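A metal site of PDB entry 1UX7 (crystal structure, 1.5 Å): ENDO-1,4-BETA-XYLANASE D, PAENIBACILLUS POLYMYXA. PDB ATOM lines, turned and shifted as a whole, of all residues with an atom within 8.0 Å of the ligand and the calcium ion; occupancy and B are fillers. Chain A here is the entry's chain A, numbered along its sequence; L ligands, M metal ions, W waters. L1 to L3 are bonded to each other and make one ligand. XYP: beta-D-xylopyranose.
N of Tyr 29 sits at hydrogen-bond distance from OD2 of Asp 33 (2.8 Å). The backbone NH of Asp 110 sits at hydrogen-bond distance from the side-chain hydroxyl of Ser 55 (2.9 Å). OD2 of Asp 105 sits at hydrogen-bond distance from N of Gly 107 (3.4 Å). The backbone NH (N) of Asp 105 sits at hydrogen-bond distance from the side-chain amide oxygen (OD1) of Asn 31, 2.8 Å away. The backbone NH (N) of Tyr 15 sits at hydrogen-bond distance from the side-chain carboxylate (OD1) of Asp 33.
Water W3 lies within hydrogen-bond range of the side-chain carboxylate of Asp 110 (2.7 Å) and an oxygen (O4) of XYP L2 (3.4 Å). Water W2 lies within hydrogen-bond range of an oxygen (O4) of XYP L3 (2.7 Å) and the backbone carbonyl oxygen (O) of Tyr 15 (2.7 Å). Water W4 lies within hydrogen-bond range of the side-chain carboxylate of Asp 105 (2.8 Å), the backbone NH of Asn 31 (3.0 Å) and an oxygen (O1) of XYP L1 (3.3 Å).
Merely in contact with the ligand: Tyr 15 (3.6 Å) and Gly 107 (3.5 Å). The nearest printed residue that does not touch the ligand is Ala 30 (4.2 Å).
O of Tyr 29 binds the calcium ion. OD1 of Asp 110 is bound to the calcium ion (2.4 Å). The side-chain carboxylate (OD1) of Asp 105 is bound to the calcium ion, at 2.4 Å. O of Trp 109 binds the calcium ion (2.4 Å). Water W1 binds the calcium ion (2.4 Å). An oxygen (O2) of XYP L2 binds the calcium ion (2.5 Å). O3 of XYP L2 is bound to the calcium ion. The calcium ion has seven donor atoms within binding distance.
The nearest printed residue that does not touch the calcium ion is Ala 30 (4.6 Å).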
ATOM      1  N   THR A  14      -4.150   1.092   4.169  1.00  0.00           N
ATOM      2  CA  THR A  14      -4.958   0.156   3.396  1.00  0.00           C
ATOM      3  C   THR A  14      -5.541   0.703   2.094  1.00  0.00           C
ATOM      4  O   THR A  14      -5.497   0.020   1.064  1.00  0.00           O
ATOM      5  CB  THR A  14      -6.077  -0.373   4.299  1.00  0.00           C
ATOM      6  OG1 THR A  14      -5.492  -1.014   5.434  1.00  0.00           O
ATOM      7  CG2 THR A  14      -6.881  -1.489   3.596  1.00  0.00           C
ATOM      8  N   TYR A  15      -6.085   1.925   2.134  1.00  0.00           N
ATOM      9  CA  TYR A  15      -6.891   2.422   1.019  1.00  0.00           C
ATOM     10  C   TYR A  15      -6.391   3.701   0.355  1.00  0.00           C
ATOM     11  O   TYR A  15      -6.853   4.041  -0.723  1.00  0.00           O
ATOM     12  CB  TYR A  15      -8.327   2.693   1.494  1.00  0.00           C
ATOM     13  CG  TYR A  15      -9.040   1.481   2.010  1.00  0.00           C
ATOM     14  CD1 TYR A  15      -9.437   0.481   1.145  1.00  0.00           C
ATOM     15  CD2 TYR A  15      -9.321   1.341   3.357  1.00  0.00           C
ATOM     16  CE1 TYR A  15     -10.108  -0.638   1.603  1.00  0.00           C
ATOM     17  CE2 TYR A  15      -9.977   0.228   3.835  1.00  0.00           C
ATOM     18  CZ  TYR A  15     -10.359  -0.764   2.955  1.00  0.00           C
ATOM     19  OH  TYR A  15     -11.028  -1.881   3.438  1.00  0.00           O
ATOM     20  N   ALA A  16      -5.460   4.410   0.976  1.00  0.00           N
ATOM     21  CA  ALA A  16      -5.060   5.718   0.451  1.00  0.00           C
ATOM     22  C   ALA A  16      -4.609   5.626  -0.999  1.00  0.00           C
ATOM     23  O   ALA A  16      -3.906   4.672  -1.404  1.00  0.00           O
ATOM     24  CB  ALA A  16      -3.980   6.316   1.281  1.00  0.00           C
ATOM     25  N   GLY A  17      -4.999   6.611  -1.795  1.00  0.00           N
ATOM     26  CA  GLY A  17      -4.602   6.700  -3.171  1.00  0.00           C
ATOM     27  C   GLY A  17      -4.805   8.046  -3.785  1.00  0.00           C
ATOM     28  O   GLY A  17      -5.527   8.877  -3.269  1.00  0.00           O
ATOM     29  N   ALA A  27      -6.625  10.891  -1.533  1.00  0.00           N
ATOM     30  CA  ALA A  27      -7.745  10.557  -0.681  1.00  0.00           C
ATOM     31  C   ALA A  27      -7.296   9.633   0.439  1.00  0.00           C
ATOM     32  O   ALA A  27      -6.575   8.646   0.199  1.00  0.00           O
ATOM     33  CB  ALA A  27      -8.847   9.921  -1.478  1.00  0.00           C
ATOM     34  N   LEU A  28      -7.734   9.967   1.646  1.00  0.00           N
ATOM     35  CA  LEU A  28      -7.569   9.145   2.829  1.00  0.00           C
ATOM     36  C   LEU A  28      -8.954   8.665   3.212  1.00  0.00           C
ATOM     37  O   LEU A  28      -9.888   9.448   3.356  1.00  0.00           O
ATOM     38  CB  LEU A  28      -6.912   9.943   3.947  1.00  0.00           C
ATOM     39  CG  LEU A  28      -5.667  10.753   3.618  1.00  0.00           C
ATOM     40  CD1 LEU A  28      -5.212  11.466   4.858  1.00  0.00           C
ATOM     41  CD2 LEU A  28      -4.573   9.876   3.062  1.00  0.00           C
ATOM     42  N   TYR A  29      -9.124   7.342   3.339  1.00  0.00           N
ATOM     43  CA  TYR A  29     -10.433   6.727   3.492  1.00  0.00           C
ATOM     44  C   TYR A  29     -10.654   6.140   4.888  1.00  0.00           C
ATOM     45  O   TYR A  29     -11.739   6.308   5.507  1.00  0.00           O
ATOM     46  CB  TYR A  29     -10.601   5.611   2.446  1.00  0.00           C
ATOM     47  CG  TYR A  29     -10.504   6.061   1.002  1.00  0.00           C
ATOM     48  CD1 TYR A  29     -11.648   6.503   0.320  1.00  0.00           C
ATOM     49  CD2 TYR A  29      -9.308   6.034   0.313  1.00  0.00           C
ATOM     50  CE1 TYR A  29     -11.575   6.907  -0.991  1.00  0.00           C
ATOM     51  CE2 TYR A  29      -9.244   6.406  -1.005  1.00  0.00           C
ATOM     52  CZ  TYR A  29     -10.377   6.849  -1.659  1.00  0.00           C
ATOM     53  OH  TYR A  29     -10.291   7.257  -2.977  1.00  0.00           O
ATOM     54  N   ALA A  30      -9.642   5.429   5.391  1.00  0.00           N
ATOM     55  CA  ALA A  30      -9.731   4.742   6.673  1.00  0.00           C
ATOM     56  C   ALA A  30      -8.641   5.185   7.620  1.00  0.00           C
ATOM     57  O   ALA A  30      -7.618   5.728   7.185  1.00  0.00           O
ATOM     58  CB  ALA A  30      -9.606   3.216   6.453  1.00  0.00           C
ATOM     59  N   ASN A  31      -8.812   4.918   8.914  1.00  0.00           N
ATOM     60  CA  ASN A  31      -7.776   5.203   9.886  1.00  0.00           C
ATOM     61  C   ASN A  31      -6.472   4.520   9.502  1.00  0.00           C
ATOM     62  O   ASN A  31      -6.471   3.417   8.981  1.00  0.00           O
ATOM     63  CB  ASN A  31      -8.211   4.821  11.301  1.00  0.00           C
ATOM     64  CG  ASN A  31      -9.295   5.755  11.828  1.00  0.00           C
ATOM     65  OD1 ASN A  31      -9.335   6.938  11.474  1.00  0.00           O
ATOM     66  ND2 ASN A  31     -10.170   5.228  12.667  1.00  0.00           N
ATOM     67  N   ASP A  33      -4.622   5.587   7.129  1.00  0.00           N
ATOM     68  CA  ASP A  33      -4.301   6.070   5.778  1.00  0.00           C
ATOM     69  C   ASP A  33      -3.547   7.383   6.011  1.00  0.00           C
ATOM     70  O   ASP A  33      -3.897   8.164   6.921  1.00  0.00           O
ATOM     71  CB  ASP A  33      -5.537   6.376   4.922  1.00  0.00           C
ATOM     72  CG  ASP A  33      -6.132   5.164   4.225  1.00  0.00           C
ATOM     73  OD1 ASP A  33      -5.509   4.055   4.171  1.00  0.00           O
ATOM     74  OD2 ASP A  33      -7.240   5.246   3.635  1.00  0.00           O
ATOM     75  N   SER A  55     -15.328  14.274   1.375  1.00  0.00           N
ATOM     76  CA  SER A  55     -16.030  13.548   0.331  1.00  0.00           C
ATOM     77  C   SER A  55     -17.521  13.858   0.320  1.00  0.00           C
ATOM     78  O   SER A  55     -18.211  13.549  -0.647  1.00  0.00           O
ATOM     79  CB  SER A  55     -15.816  12.046   0.533  1.00  0.00           C
ATOM     80  OG  SER A  55     -16.348  11.640   1.764  1.00  0.00           O
ATOM     81  N   ASN A  56     -18.008  14.442   1.404  1.00  0.00           N
ATOM     82  CA  ASN A  56     -19.443  14.737   1.475  1.00  0.00           C
ATOM     83  C   ASN A  56     -19.706  15.927   2.394  1.00  0.00           C
ATOM     84  O   ASN A  56     -18.803  16.719   2.697  1.00  0.00           O
ATOM     85  CB  ASN A  56     -20.195  13.486   1.915  1.00  0.00           C
ATOM     86  CG  ASN A  56     -19.724  12.939   3.236  1.00  0.00           C
ATOM     87  OD1 ASN A  56     -19.296  13.683   4.124  1.00  0.00           O
ATOM     88  ND2 ASN A  56     -19.777  11.598   3.361  1.00  0.00           N
ATOM     89  N   LEU A 102      -5.242   9.966   8.970  1.00  0.00           N
ATOM     90  CA  LEU A 102      -6.562   9.783   9.579  1.00  0.00           C
ATOM     91  C   LEU A 102      -6.490   8.949  10.817  1.00  0.00           C
ATOM     92  O   LEU A 102      -5.889   7.866  10.801  1.00  0.00           O
ATOM     93  CB  LEU A 102      -7.508   9.075   8.632  1.00  0.00           C
ATOM     94  CG  LEU A 102      -7.868   9.787   7.366  1.00  0.00           C
ATOM     95  CD1 LEU A 102      -9.076   9.118   6.724  1.00  0.00           C
ATOM     96  CD2 LEU A 102      -8.131  11.281   7.649  1.00  0.00           C
ATOM     97  N   SER A 104      -9.590   9.482  12.994  1.00  0.00           N
ATOM     98  CA  SER A 104     -10.945   9.618  13.505  1.00  0.00           C
ATOM     99  C   SER A 104     -12.032   9.256  12.492  1.00  0.00           C
ATOM    100  O   SER A 104     -13.215   9.594  12.693  1.00  0.00           O
ATOM    101  CB  SER A 104     -11.136  11.031  14.007  1.00  0.00           C
ATOM    102  OG  SER A 104     -11.150  11.901  12.911  1.00  0.00           O
ATOM    103  N   ASP A 105     -11.664   8.557  11.441  1.00  0.00           N
ATOM    104  CA  ASP A 105     -12.632   8.016  10.503  1.00  0.00           C
ATOM    105  C   ASP A 105     -13.574   7.076  11.270  1.00  0.00           C
ATOM    106  O   ASP A 105     -13.153   6.344  12.202  1.00  0.00           O
ATOM    107  CB  ASP A 105     -11.955   7.288   9.350  1.00  0.00           C
ATOM    108  CG  ASP A 105     -12.928   6.610   8.453  1.00  0.00           C
ATOM    109  OD1 ASP A 105     -13.548   7.262   7.576  1.00  0.00           O
ATOM    110  OD2 ASP A 105     -13.158   5.382   8.543  1.00  0.00           O
ATOM    111  N   ASP A 106     -14.839   7.139  10.893  1.00  0.00           N
ATOM    112  CA  ASP A 106     -15.906   6.292  11.474  1.00  0.00           C
ATOM    113  C   ASP A 106     -16.899   5.804  10.425  1.00  0.00           C
ATOM    114  O   ASP A 106     -18.050   5.409  10.779  1.00  0.00           O
ATOM    115  CB  ASP A 106     -16.588   7.003  12.640  1.00  0.00           C
ATOM    116  CG  ASP A 106     -17.234   8.326  12.241  1.00  0.00           C
ATOM    117  OD1 ASP A 106     -17.365   8.589  11.025  1.00  0.00           O
ATOM    118  OD2 ASP A 106     -17.614   9.195  13.088  1.00  0.00           O
ATOM    119  N   GLY A 107     -16.483   5.738   9.170  1.00  0.00           N
ATOM    120  CA  GLY A 107     -17.305   5.274   8.088  1.00  0.00           C
ATOM    121  C   GLY A 107     -18.325   6.315   7.627  1.00  0.00           C
ATOM    122  O   GLY A 107     -19.291   5.964   6.972  1.00  0.00           O
ATOM    123  N   THR A 108     -18.130   7.586   7.981  1.00  0.00           N
ATOM    124  CA  THR A 108     -19.113   8.604   7.535  1.00  0.00           C
ATOM    125  C   THR A 108     -18.573   9.627   6.527  1.00  0.00           C
ATOM    126  O   THR A 108     -19.353  10.429   6.031  1.00  0.00           O
ATOM    127  CB  THR A 108     -19.772   9.362   8.730  1.00  0.00           C
ATOM    128  OG1 THR A 108     -18.825  10.113   9.490  1.00  0.00           O
ATOM    129  CG2 THR A 108     -20.429   8.420   9.745  1.00  0.00           C
ATOM    130  N   TRP A 109     -17.265   9.605   6.282  1.00  0.00           N
ATOM    131  CA  TRP A 109     -16.614  10.536   5.317  1.00  0.00           C
ATOM    132  C   TRP A 109     -15.249  10.009   4.944  1.00  0.00           C
ATOM    133  O   TRP A 109     -14.720   9.075   5.581  1.00  0.00           O
ATOM    134  CB  TRP A 109     -16.468  11.964   5.886  1.00  0.00           C
ATOM    135  CG  TRP A 109     -15.943  12.032   7.262  1.00  0.00           C
ATOM    136  CD1 TRP A 109     -16.674  12.165   8.391  1.00  0.00           C
ATOM    137  CD2 TRP A 109     -14.571  11.905   7.693  1.00  0.00           C
ATOM    138  NE1 TRP A 109     -15.868  12.160   9.498  1.00  0.00           N
ATOM    139  CE2 TRP A 109     -14.562  12.005   9.100  1.00  0.00           C
ATOM    140  CE3 TRP A 109     -13.345  11.748   7.036  1.00  0.00           C
ATOM    141  CZ2 TRP A 109     -13.405  11.916   9.854  1.00  0.00           C
ATOM    142  CZ3 TRP A 109     -12.184  11.685   7.780  1.00  0.00           C
ATOM    143  CH2 TRP A 109     -12.227  11.760   9.180  1.00  0.00           C
ATOM    144  N   ASP A 110     -14.708  10.598   3.879  1.00  0.00           N
ATOM    145  CA  ASP A 110     -13.310  10.450   3.492  1.00  0.00           C
ATOM    146  C   ASP A 110     -12.699  11.854   3.407  1.00  0.00           C
ATOM    147  O   ASP A 110     -13.432  12.826   3.280  1.00  0.00           O
ATOM    148  CB  ASP A 110     -13.201   9.752   2.145  1.00  0.00           C
ATOM    149  CG  ASP A 110     -13.933   8.432   2.123  1.00  0.00           C
ATOM    150  OD1 ASP A 110     -13.752   7.693   3.107  1.00  0.00           O
ATOM    151  OD2 ASP A 110     -14.670   8.057   1.168  1.00  0.00           O
ATOM    152  N   ALA A 111     -11.376  11.926   3.497  1.00  0.00           N
ATOM    153  CA  ALA A 111     -10.658  13.190   3.465  1.00  0.00           C
ATOM    154  C   ALA A 111      -9.858  13.284   2.175  1.00  0.00           C
ATOM    155  O   ALA A 111      -9.154  12.348   1.802  1.00  0.00           O
ATOM    156  CB  ALA A 111      -9.740  13.297   4.651  1.00  0.00           C
HETATM  157  O1  XYP L   1     -13.450   2.101   7.570  1.00  0.00           O
HETATM  158  C1  XYP L   1     -14.409   1.801   8.574  1.00  0.00           C
HETATM  159  C1  XYP L   2     -13.997   2.103   6.230  1.00  0.00           C
HETATM  160  C2  XYP L   2     -13.781   3.474   5.600  1.00  0.00           C
HETATM  161  C3  XYP L   2     -14.221   3.497   4.134  1.00  0.00           C
HETATM  162  C4  XYP L   2     -13.575   2.359   3.362  1.00  0.00           C
HETATM  163  C5  XYP L   2     -13.864   1.069   4.117  1.00  0.00           C
HETATM  164  O2  XYP L   2     -14.416   4.520   6.335  1.00  0.00           O
HETATM  165  O3  XYP L   2     -13.866   4.736   3.551  1.00  0.00           O
HETATM  166  O4  XYP L   2     -14.111   2.286   2.048  1.00  0.00           O
HETATM  167  O5  XYP L   2     -13.371   1.189   5.436  1.00  0.00           O
HETATM  168  C1  XYP L   3     -13.157   1.972   1.030  1.00  0.00           C
HETATM  169  C2  XYP L   3     -13.935   1.391  -0.125  1.00  0.00           C
HETATM  170  C3  XYP L   3     -13.071   1.158  -1.368  1.00  0.00           C
HETATM  171  C4  XYP L   3     -12.259   2.427  -1.675  1.00  0.00           C
HETATM  172  C5  XYP L   3     -11.563   2.877  -0.412  1.00  0.00           C
HETATM  173  O2  XYP L   3     -14.556   0.203   0.308  1.00  0.00           O
HETATM  174  O3  XYP L   3     -13.927   0.794  -2.440  1.00  0.00           O
HETATM  175  O4  XYP L   3     -11.249   2.260  -2.665  1.00  0.00           O
HETATM  176  O5  XYP L   3     -12.524   3.088   0.591  1.00  0.00           O
HETATM  177 CA    CA M   1     -14.017   6.798   5.270  1.00  0.00          CA
HETATM  178  O   HOH W   1     -16.428   6.571   5.019  1.00  0.00           O
HETATM  179  O   HOH W   2      -8.661   2.688  -2.239  1.00  0.00           O
HETATM  180  O   HOH W   3     -15.200   5.436   1.515  1.00  0.00           O
HETATM  181  O   HOH W   4     -11.373   3.597   9.671  1.00  0.00           O
